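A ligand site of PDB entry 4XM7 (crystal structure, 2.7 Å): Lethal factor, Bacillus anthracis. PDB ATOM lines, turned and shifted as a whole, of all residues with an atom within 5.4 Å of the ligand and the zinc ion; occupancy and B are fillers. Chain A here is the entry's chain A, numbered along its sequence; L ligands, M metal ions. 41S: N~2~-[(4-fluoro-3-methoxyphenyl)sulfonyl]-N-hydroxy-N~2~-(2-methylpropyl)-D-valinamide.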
ATOM      1  N   ASP A  67      -5.916  -6.058  -9.829  1.00  0.00           N
ATOM      2  CA  ASP A  67      -5.409  -5.380 -11.017  1.00  0.00           C
ATOM      3  C   ASP A  67      -4.494  -6.265 -11.861  1.00  0.00           C
ATOM      4  O   ASP A  67      -4.235  -5.955 -13.027  1.00  0.00           O
ATOM      5  CB  ASP A  67      -4.654  -4.105 -10.591  1.00  0.00           C
ATOM      6  CG  ASP A  67      -3.573  -4.378  -9.552  1.00  0.00           C
ATOM      7  OD1 ASP A  67      -2.859  -5.395  -9.665  1.00  0.00           O
ATOM      8  OD2 ASP A  67      -3.424  -3.558  -8.628  1.00  0.00           O
ATOM      9  N   VAL A 392       3.072  -9.783 -13.352  1.00  0.00           N
ATOM     10  CA  VAL A 392       1.852  -8.983 -13.436  1.00  0.00           C
ATOM     11  C   VAL A 392       1.372  -8.874 -14.865  1.00  0.00           C
ATOM     12  O   VAL A 392       2.150  -8.584 -15.773  1.00  0.00           O
ATOM     13  CB  VAL A 392       2.077  -7.553 -12.877  1.00  0.00           C
ATOM     14  CG1 VAL A 392       0.834  -6.696 -13.076  1.00  0.00           C
ATOM     15  CG2 VAL A 392       2.468  -7.605 -11.404  1.00  0.00           C
ATOM     16  N   SER A 394      -1.334  -6.515 -16.882  1.00  0.00           N
ATOM     17  CA  SER A 394      -2.176  -5.334 -16.827  1.00  0.00           C
ATOM     18  C   SER A 394      -1.978  -4.614 -18.155  1.00  0.00           C
ATOM     19  O   SER A 394      -1.159  -5.043 -18.958  1.00  0.00           O
ATOM     20  CB  SER A 394      -1.813  -4.452 -15.639  1.00  0.00           C
ATOM     21  OG  SER A 394      -0.417  -4.176 -15.617  1.00  0.00           O
ATOM     22  N   LYS A 395      -2.719  -3.541 -18.385  1.00  0.00           N
ATOM     23  CA  LYS A 395      -2.584  -2.836 -19.656  1.00  0.00           C
ATOM     24  C   LYS A 395      -1.201  -2.192 -19.756  1.00  0.00           C
ATOM     25  O   LYS A 395      -0.647  -2.078 -20.850  1.00  0.00           O
ATOM     26  CB  LYS A 395      -3.678  -1.783 -19.819  1.00  0.00           C
ATOM     27  CG  LYS A 395      -3.556  -0.977 -21.101  1.00  0.00           C
ATOM     28  CD  LYS A 395      -4.906  -0.533 -21.630  1.00  0.00           C
ATOM     29  CE  LYS A 395      -4.766   0.101 -23.000  1.00  0.00           C
ATOM     30  NZ  LYS A 395      -4.280  -0.880 -24.015  1.00  0.00           N
ATOM     31  N   GLY A 396      -0.642  -1.793 -18.619  1.00  0.00           N
ATOM     32  CA  GLY A 396       0.651  -1.142 -18.596  1.00  0.00           C
ATOM     33  C   GLY A 396       1.418  -1.342 -17.320  1.00  0.00           C
ATOM     34  O   GLY A 396       0.877  -1.762 -16.298  1.00  0.00           O
ATOM     35  N   LEU A 397       2.711  -1.009 -17.365  1.00  0.00           N
ATOM     36  CA  LEU A 397       3.602  -1.214 -16.225  1.00  0.00           C
ATOM     37  C   LEU A 397       4.852  -0.358 -16.367  1.00  0.00           C
ATOM     38  O   LEU A 397       5.303  -0.077 -17.479  1.00  0.00           O
ATOM     39  CB  LEU A 397       3.979  -2.696 -16.120  1.00  0.00           C
ATOM     40  CG  LEU A 397       4.148  -3.312 -14.740  1.00  0.00           C
ATOM     41  CD1 LEU A 397       2.843  -3.251 -13.966  1.00  0.00           C
ATOM     42  CD2 LEU A 397       4.639  -4.756 -14.856  1.00  0.00           C
ATOM     43  N   TYR A 398       5.415   0.063 -15.232  1.00  0.00           N
ATOM     44  CA  TYR A 398       6.765   0.600 -15.237  1.00  0.00           C
ATOM     45  C   TYR A 398       7.653  -0.289 -14.390  1.00  0.00           C
ATOM     46  O   TYR A 398       7.347  -0.572 -13.226  1.00  0.00           O
ATOM     47  CB  TYR A 398       6.813   2.040 -14.713  1.00  0.00           C
ATOM     48  CG  TYR A 398       8.237   2.520 -14.526  1.00  0.00           C
ATOM     49  CD1 TYR A 398       9.027   2.824 -15.621  1.00  0.00           C
ATOM     50  CD2 TYR A 398       8.791   2.645 -13.258  1.00  0.00           C
ATOM     51  CE1 TYR A 398      10.344   3.251 -15.465  1.00  0.00           C
ATOM     52  CE2 TYR A 398      10.106   3.070 -13.093  1.00  0.00           C
ATOM     53  CZ  TYR A 398      10.867   3.369 -14.196  1.00  0.00           C
ATOM     54  OH  TYR A 398      12.163   3.790 -14.047  1.00  0.00           O
ATOM     55  N   LEU A 407       3.539  -1.378 -22.428  1.00  0.00           N
ATOM     56  CA  LEU A 407       2.161  -1.037 -22.761  1.00  0.00           C
ATOM     57  C   LEU A 407       1.526  -2.089 -23.646  1.00  0.00           C
ATOM     58  O   LEU A 407       1.926  -2.283 -24.794  1.00  0.00           O
ATOM     59  CB  LEU A 407       2.105   0.336 -23.440  1.00  0.00           C
ATOM     60  CG  LEU A 407       0.754   1.033 -23.265  1.00  0.00           C
ATOM     61  CD1 LEU A 407       0.584   1.422 -21.814  1.00  0.00           C
ATOM     62  CD2 LEU A 407       0.646   2.255 -24.160  1.00  0.00           C
ATOM     63  N   LYS A 412      -7.940  -3.808 -21.781  1.00  0.00           N
ATOM     64  CA  LYS A 412      -8.669  -2.620 -21.342  1.00  0.00           C
ATOM     65  C   LYS A 412      -8.119  -2.096 -20.022  1.00  0.00           C
ATOM     66  O   LYS A 412      -7.661  -2.862 -19.184  1.00  0.00           O
ATOM     67  CB  LYS A 412     -10.161  -2.939 -21.194  1.00  0.00           C
ATOM     68  CG  LYS A 412     -11.022  -1.747 -20.815  1.00  0.00           C
ATOM     69  CD  LYS A 412     -12.504  -2.129 -20.731  1.00  0.00           C
ATOM     70  CE  LYS A 412     -13.359  -0.936 -20.329  1.00  0.00           C
ATOM     71  NZ  LYS A 412     -14.815  -1.280 -20.237  1.00  0.00           N
ATOM     72  N   GLY A 413      -8.181  -0.786 -19.838  1.00  0.00           N
ATOM     73  CA  GLY A 413      -7.652  -0.177 -18.623  1.00  0.00           C
ATOM     74  C   GLY A 413      -8.657  -0.073 -17.498  1.00  0.00           C
ATOM     75  O   GLY A 413      -9.866  -0.035 -17.727  1.00  0.00           O
ATOM     76  N   VAL A 414      -8.143  -0.046 -16.273  1.00  0.00           N
ATOM     77  CA  VAL A 414      -8.986   0.162 -15.097  1.00  0.00           C
ATOM     78  C   VAL A 414      -9.468   1.605 -15.099  1.00  0.00           C
ATOM     79  O   VAL A 414      -8.747   2.518 -14.698  1.00  0.00           O
ATOM     80  CB  VAL A 414      -8.222  -0.148 -13.784  1.00  0.00           C
ATOM     81  CG1 VAL A 414      -9.020   0.317 -12.563  1.00  0.00           C
ATOM     82  CG2 VAL A 414      -7.914  -1.629 -13.693  1.00  0.00           C
ATOM     83  N   LEU A 416      -9.999   4.109 -17.477  1.00  0.00           N
ATOM     84  CA  LEU A 416      -9.115   5.113 -18.058  1.00  0.00           C
ATOM     85  C   LEU A 416      -9.429   5.325 -19.523  1.00  0.00           C
ATOM     86  O   LEU A 416      -9.670   4.372 -20.266  1.00  0.00           O
ATOM     87  CB  LEU A 416      -7.650   4.712 -17.878  1.00  0.00           C
ATOM     88  CG  LEU A 416      -6.726   5.880 -17.528  1.00  0.00           C
ATOM     89  CD1 LEU A 416      -7.095   6.416 -16.157  1.00  0.00           C
ATOM     90  CD2 LEU A 416      -5.265   5.479 -17.577  1.00  0.00           C
ATOM     91  N   ASN A 418      -7.859   6.497 -22.535  1.00  0.00           N
ATOM     92  CA  ASN A 418      -7.105   6.117 -23.714  1.00  0.00           C
ATOM     93  C   ASN A 418      -5.719   5.650 -23.304  1.00  0.00           C
ATOM     94  O   ASN A 418      -5.298   5.836 -22.163  1.00  0.00           O
ATOM     95  CB  ASN A 418      -7.001   7.164 -24.829  1.00  0.00           C
ATOM     96  CG  ASN A 418      -6.555   8.513 -24.315  1.00  0.00           C
ATOM     97  OD1 ASN A 418      -5.552   8.630 -23.612  1.00  0.00           O
ATOM     98  ND2 ASN A 418      -7.317   9.552 -24.649  1.00  0.00           N
ATOM     99  N   ASP A 419      -5.013   5.026 -24.244  1.00  0.00           N
ATOM    100  CA  ASP A 419      -3.660   4.545 -24.019  1.00  0.00           C
ATOM    101  C   ASP A 419      -2.714   5.698 -23.691  1.00  0.00           C
ATOM    102  O   ASP A 419      -1.814   5.554 -22.864  1.00  0.00           O
ATOM    103  CB  ASP A 419      -3.134   3.791 -25.249  1.00  0.00           C
ATOM    104  CG  ASP A 419      -4.014   2.617 -25.624  1.00  0.00           C
ATOM    105  OD1 ASP A 419      -5.223   2.647 -25.283  1.00  0.00           O
ATOM    106  OD2 ASP A 419      -3.502   1.672 -26.253  1.00  0.00           O
ATOM    107  N   GLU A 421      -3.155   8.521 -22.110  1.00  0.00           N
ATOM    108  CA  GLU A 421      -3.223   8.967 -20.725  1.00  0.00           C
ATOM    109  C   GLU A 421      -2.529   7.966 -19.810  1.00  0.00           C
ATOM    110  O   GLU A 421      -1.889   8.328 -18.829  1.00  0.00           O
ATOM    111  CB  GLU A 421      -4.667   9.175 -20.276  1.00  0.00           C
ATOM    112  CG  GLU A 421      -5.313  10.438 -20.841  1.00  0.00           C
ATOM    113  CD  GLU A 421      -6.590  10.823 -20.110  1.00  0.00           C
ATOM    114  OE1 GLU A 421      -7.305   9.919 -19.641  1.00  0.00           O
ATOM    115  OE2 GLU A 421      -6.880  12.028 -20.012  1.00  0.00           O
ATOM    116  N   GLY A 422      -2.640   6.683 -20.163  1.00  0.00           N
ATOM    117  CA  GLY A 422      -2.003   5.641 -19.382  1.00  0.00           C
ATOM    118  C   GLY A 422      -0.498   5.626 -19.502  1.00  0.00           C
ATOM    119  O   GLY A 422       0.204   5.266 -18.555  1.00  0.00           O
ATOM    120  N   PHE A 423       0.022   6.026 -20.665  1.00  0.00           N
ATOM    121  CA  PHE A 423       1.462   6.102 -20.865  1.00  0.00           C
ATOM    122  C   PHE A 423       2.060   7.213 -20.012  1.00  0.00           C
ATOM    123  O   PHE A 423       3.140   7.047 -19.433  1.00  0.00           O
ATOM    124  CB  PHE A 423       1.801   6.347 -22.339  1.00  0.00           C
ATOM    125  CG  PHE A 423       3.284   6.360 -22.616  1.00  0.00           C
ATOM    126  CD1 PHE A 423       3.970   5.185 -22.844  1.00  0.00           C
ATOM    127  CD2 PHE A 423       3.979   7.566 -22.649  1.00  0.00           C
ATOM    128  CE1 PHE A 423       5.327   5.201 -23.093  1.00  0.00           C
ATOM    129  CE2 PHE A 423       5.345   7.581 -22.897  1.00  0.00           C
ATOM    130  CZ  PHE A 423       6.018   6.394 -23.121  1.00  0.00           C
ATOM    131  N   HIS A 425       0.855   8.274 -17.255  1.00  0.00           N
ATOM    132  CA  HIS A 425       0.844   7.704 -15.920  1.00  0.00           C
ATOM    133  C   HIS A 425       2.106   6.881 -15.672  1.00  0.00           C
ATOM    134  O   HIS A 425       2.750   7.017 -14.630  1.00  0.00           O
ATOM    135  CB  HIS A 425      -0.404   6.843 -15.736  1.00  0.00           C
ATOM    136  CG  HIS A 425      -0.394   5.995 -14.495  1.00  0.00           C
ATOM    137  ND1 HIS A 425      -1.223   6.243 -13.432  1.00  0.00           N
ATOM    138  CD2 HIS A 425       0.320   4.894 -14.182  1.00  0.00           C
ATOM    139  CE1 HIS A 425      -1.011   5.326 -12.494  1.00  0.00           C
ATOM    140  NE2 HIS A 425      -0.080   4.510 -12.922  1.00  0.00           N
ATOM    141  N   GLU A 426       2.462   6.035 -16.636  1.00  0.00           N
ATOM    142  CA  GLU A 426       3.652   5.206 -16.525  1.00  0.00           C
ATOM    143  C   GLU A 426       4.917   6.063 -16.501  1.00  0.00           C
ATOM    144  O   GLU A 426       5.850   5.786 -15.757  1.00  0.00           O
ATOM    145  CB  GLU A 426       3.732   4.194 -17.661  1.00  0.00           C
ATOM    146  CG  GLU A 426       2.527   3.260 -17.753  1.00  0.00           C
ATOM    147  CD  GLU A 426       2.419   2.311 -16.583  1.00  0.00           C
ATOM    148  OE1 GLU A 426       1.407   1.592 -16.503  1.00  0.00           O
ATOM    149  OE2 GLU A 426       3.344   2.269 -15.747  1.00  0.00           O
ATOM    150  N   HIS A 429       5.776   7.273 -13.220  1.00  0.00           N
ATOM    151  CA  HIS A 429       6.549   6.343 -12.403  1.00  0.00           C
ATOM    152  C   HIS A 429       8.040   6.557 -12.587  1.00  0.00           C
ATOM    153  O   HIS A 429       8.809   6.561 -11.628  1.00  0.00           O
ATOM    154  CB  HIS A 429       6.198   4.906 -12.765  1.00  0.00           C
ATOM    155  CG  HIS A 429       4.984   4.386 -12.065  1.00  0.00           C
ATOM    156  ND1 HIS A 429       4.773   4.558 -10.710  1.00  0.00           N
ATOM    157  CD2 HIS A 429       3.927   3.678 -12.521  1.00  0.00           C
ATOM    158  CE1 HIS A 429       3.639   3.980 -10.370  1.00  0.00           C
ATOM    159  NE2 HIS A 429       3.098   3.439 -11.445  1.00  0.00           N
ATOM    160  N   TYR A 467      -8.287   4.418  -7.998  1.00  0.00           N
ATOM    161  CA  TYR A 467      -7.135   3.529  -8.089  1.00  0.00           C
ATOM    162  C   TYR A 467      -5.893   4.152  -7.460  1.00  0.00           C
ATOM    163  O   TYR A 467      -4.992   3.437  -7.026  1.00  0.00           O
ATOM    164  CB  TYR A 467      -6.826   3.169  -9.542  1.00  0.00           C
ATOM    165  CG  TYR A 467      -5.685   2.198  -9.643  1.00  0.00           C
ATOM    166  CD1 TYR A 467      -5.805   0.913  -9.123  1.00  0.00           C
ATOM    167  CD2 TYR A 467      -4.469   2.559 -10.203  1.00  0.00           C
ATOM    168  CE1 TYR A 467      -4.751   0.013  -9.185  1.00  0.00           C
ATOM    169  CE2 TYR A 467      -3.413   1.672 -10.271  1.00  0.00           C
ATOM    170  CZ  TYR A 467      -3.561   0.392  -9.756  1.00  0.00           C
ATOM    171  OH  TYR A 467      -2.527  -0.496  -9.818  1.00  0.00           O
ATOM    172  N   GLU A 474       1.465   4.504  -6.790  1.00  0.00           N
ATOM    173  CA  GLU A 474       0.335   4.661  -7.707  1.00  0.00           C
ATOM    174  C   GLU A 474      -0.293   6.046  -7.566  1.00  0.00           C
ATOM    175  O   GLU A 474      -0.691   6.648  -8.556  1.00  0.00           O
ATOM    176  CB  GLU A 474      -0.724   3.582  -7.449  1.00  0.00           C
ATOM    177  CG  GLU A 474      -0.189   2.157  -7.311  1.00  0.00           C
ATOM    178  CD  GLU A 474       0.408   1.588  -8.601  1.00  0.00           C
ATOM    179  OE1 GLU A 474       0.547   2.346  -9.582  1.00  0.00           O
ATOM    180  OE2 GLU A 474       0.729   0.386  -8.626  1.00  0.00           O
ATOM    181  N   ALA A 477       1.520   8.655  -9.352  1.00  0.00           N
ATOM    182  CA  ALA A 477       1.403   8.464 -10.796  1.00  0.00           C
ATOM    183  C   ALA A 477       0.068   8.986 -11.338  1.00  0.00           C
ATOM    184  O   ALA A 477       0.034   9.642 -12.371  1.00  0.00           O
ATOM    185  CB  ALA A 477       1.568   6.991 -11.145  1.00  0.00           C
ATOM    186  N   GLU A 478      -1.017   8.704 -10.624  1.00  0.00           N
ATOM    187  CA  GLU A 478      -2.331   9.198 -11.009  1.00  0.00           C
ATOM    188  C   GLU A 478      -2.398  10.710 -10.907  1.00  0.00           C
ATOM    189  O   GLU A 478      -2.994  11.376 -11.756  1.00  0.00           O
ATOM    190  CB  GLU A 478      -3.423   8.566 -10.159  1.00  0.00           C
ATOM    191  CG  GLU A 478      -3.793   7.150 -10.572  1.00  0.00           C
ATOM    192  CD  GLU A 478      -4.466   7.092 -11.929  1.00  0.00           C
ATOM    193  OE1 GLU A 478      -5.702   6.948 -11.979  1.00  0.00           O
ATOM    194  OE2 GLU A 478      -3.752   7.184 -12.953  1.00  0.00           O
HETATM  195  C1  41S L   1      -1.339  -0.222 -14.232  1.00  0.00           C
HETATM  196  C2  41S L   1      -0.376   0.724 -13.584  1.00  0.00           C
HETATM  197  C3  41S L   1      -5.836   2.553 -19.609  1.00  0.00           C
HETATM  198  O5  41S L   1       1.603   1.896 -13.597  1.00  0.00           O
HETATM  199  N6  41S L   1      -2.559   0.444 -14.645  1.00  0.00           N
HETATM  200  C7  41S L   1      -0.576  -1.901 -12.521  1.00  0.00           C
HETATM  201  C8  41S L   1      -2.655  -2.331 -13.872  1.00  0.00           C
HETATM  202  C10 41S L   1      -2.941   0.798 -17.135  1.00  0.00           C
HETATM  203  C11 41S L   1      -3.910   1.272 -18.025  1.00  0.00           C
HETATM  204  C12 41S L   1      -3.520   1.982 -19.152  1.00  0.00           C
HETATM  205  C13 41S L   1      -2.178   2.226 -19.401  1.00  0.00           C
HETATM  206  C14 41S L   1      -1.218   1.753 -18.513  1.00  0.00           C
HETATM  207  C15 41S L   1      -1.599   1.041 -17.384  1.00  0.00           C
HETATM  208  O17 41S L   1      -4.474   2.446 -20.020  1.00  0.00           O
HETATM  209  C19 41S L   1      -3.326   2.669 -14.825  1.00  0.00           C
HETATM  210  C18 41S L   1      -2.934   1.594 -13.828  1.00  0.00           C
HETATM  211  C28 41S L   1      -1.778  -1.273 -13.213  1.00  0.00           C
HETATM  212  N4  41S L   1       0.772   1.040 -14.207  1.00  0.00           N
HETATM  213  O3  41S L   1      -0.615   1.351 -12.292  1.00  0.00           O
HETATM  214  S7  41S L   1      -3.385  -0.013 -15.839  1.00  0.00           S
HETATM  215  O8  41S L   1      -4.775   0.215 -15.576  1.00  0.00           O
HETATM  216  O9  41S L   1      -3.167  -1.410 -16.063  1.00  0.00           O
HETATM  217  F16 41S L   1      -1.816   2.917 -20.497  1.00  0.00           F
HETATM  218  C5  41S L   1      -4.531   3.461 -14.314  1.00  0.00           C
HETATM  219  C6  41S L   1      -2.150   3.594 -15.132  1.00  0.00           C
HETATM  220 ZN    ZN M   1       0.946   2.594 -11.745  1.00  0.00          ZN
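OH of Tyr 467 sits at hydrogen-bond distance from OD2 of Asp 67 (3.4 Å).
The side-chain carboxylate (OE2) of Glu 426 lies within hydrogen-bond range of the backbone NH (N) of Tyr 398.
A ring nitrogen (ND1) of His 425 is in hydrogen-bond range of the side-chain carboxylate (OE2) of Glu 478 (2.7 Å).
The backbone carbonyl oxygen (O) of Gly 396 is in hydrogen-bond range of the side-chain hydroxyl (OG) of Ser 394, 2.8 Å away.
NZ of Lys 395 is in salt-bridge range of OD2 of Asp 419.
OE1 of Glu 426 lies within hydrogen-bond range of N of Leu 397.
The zinc ion is bound by an oxygen (O3) of the ligand (2.1 Å), an oxygen (O5) of the ligand (2.1 Å), the side-chain carboxylate of Glu 474 (2.2 Å), a ring nitrogen (NE2) of His 429 (2.3 Å) and a ring nitrogen (NE2) of His 425 (2.5 Å).
The zinc ion has five donor atoms within binding distance.
The backbone NH (N) of Lys 395 sits at hydrogen-bond distance from an oxygen (O9) of the ligand, 3.2 Å away.
A nitrogen (N4) of the ligand lies within hydrogen-bond range of the side-chain carboxylate (OE1) of Glu 426, at 2.4 Å.
O of Gly 396 lies close to N4 of the ligand, 3.5 Å away.
The backbone NH (N) of Val 414 lies within hydrogen-bond range of an oxygen (O8) of the ligand, 3.4 Å away.
Three residues have an atom within 4 Å of the zinc ion: His 425, His 429 and Glu 474.
Merely in contact with the ligand: Ser 394, Gly 422, Leu 407, Leu 416, Gly 413, Tyr 467, Asp 419, Phe 423 and Leu 397.
Hydrophobic or aromatic side chains that line the ligand: Leu 397, Leu 407, Val 414, Leu 416, His 425, His 429 and Tyr 467.
Of the 24 residues printed, 16 come within 4 Å of the ligand.
The nearest printed residue that does not touch the ligand is Glu 478 (4.04 Å).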
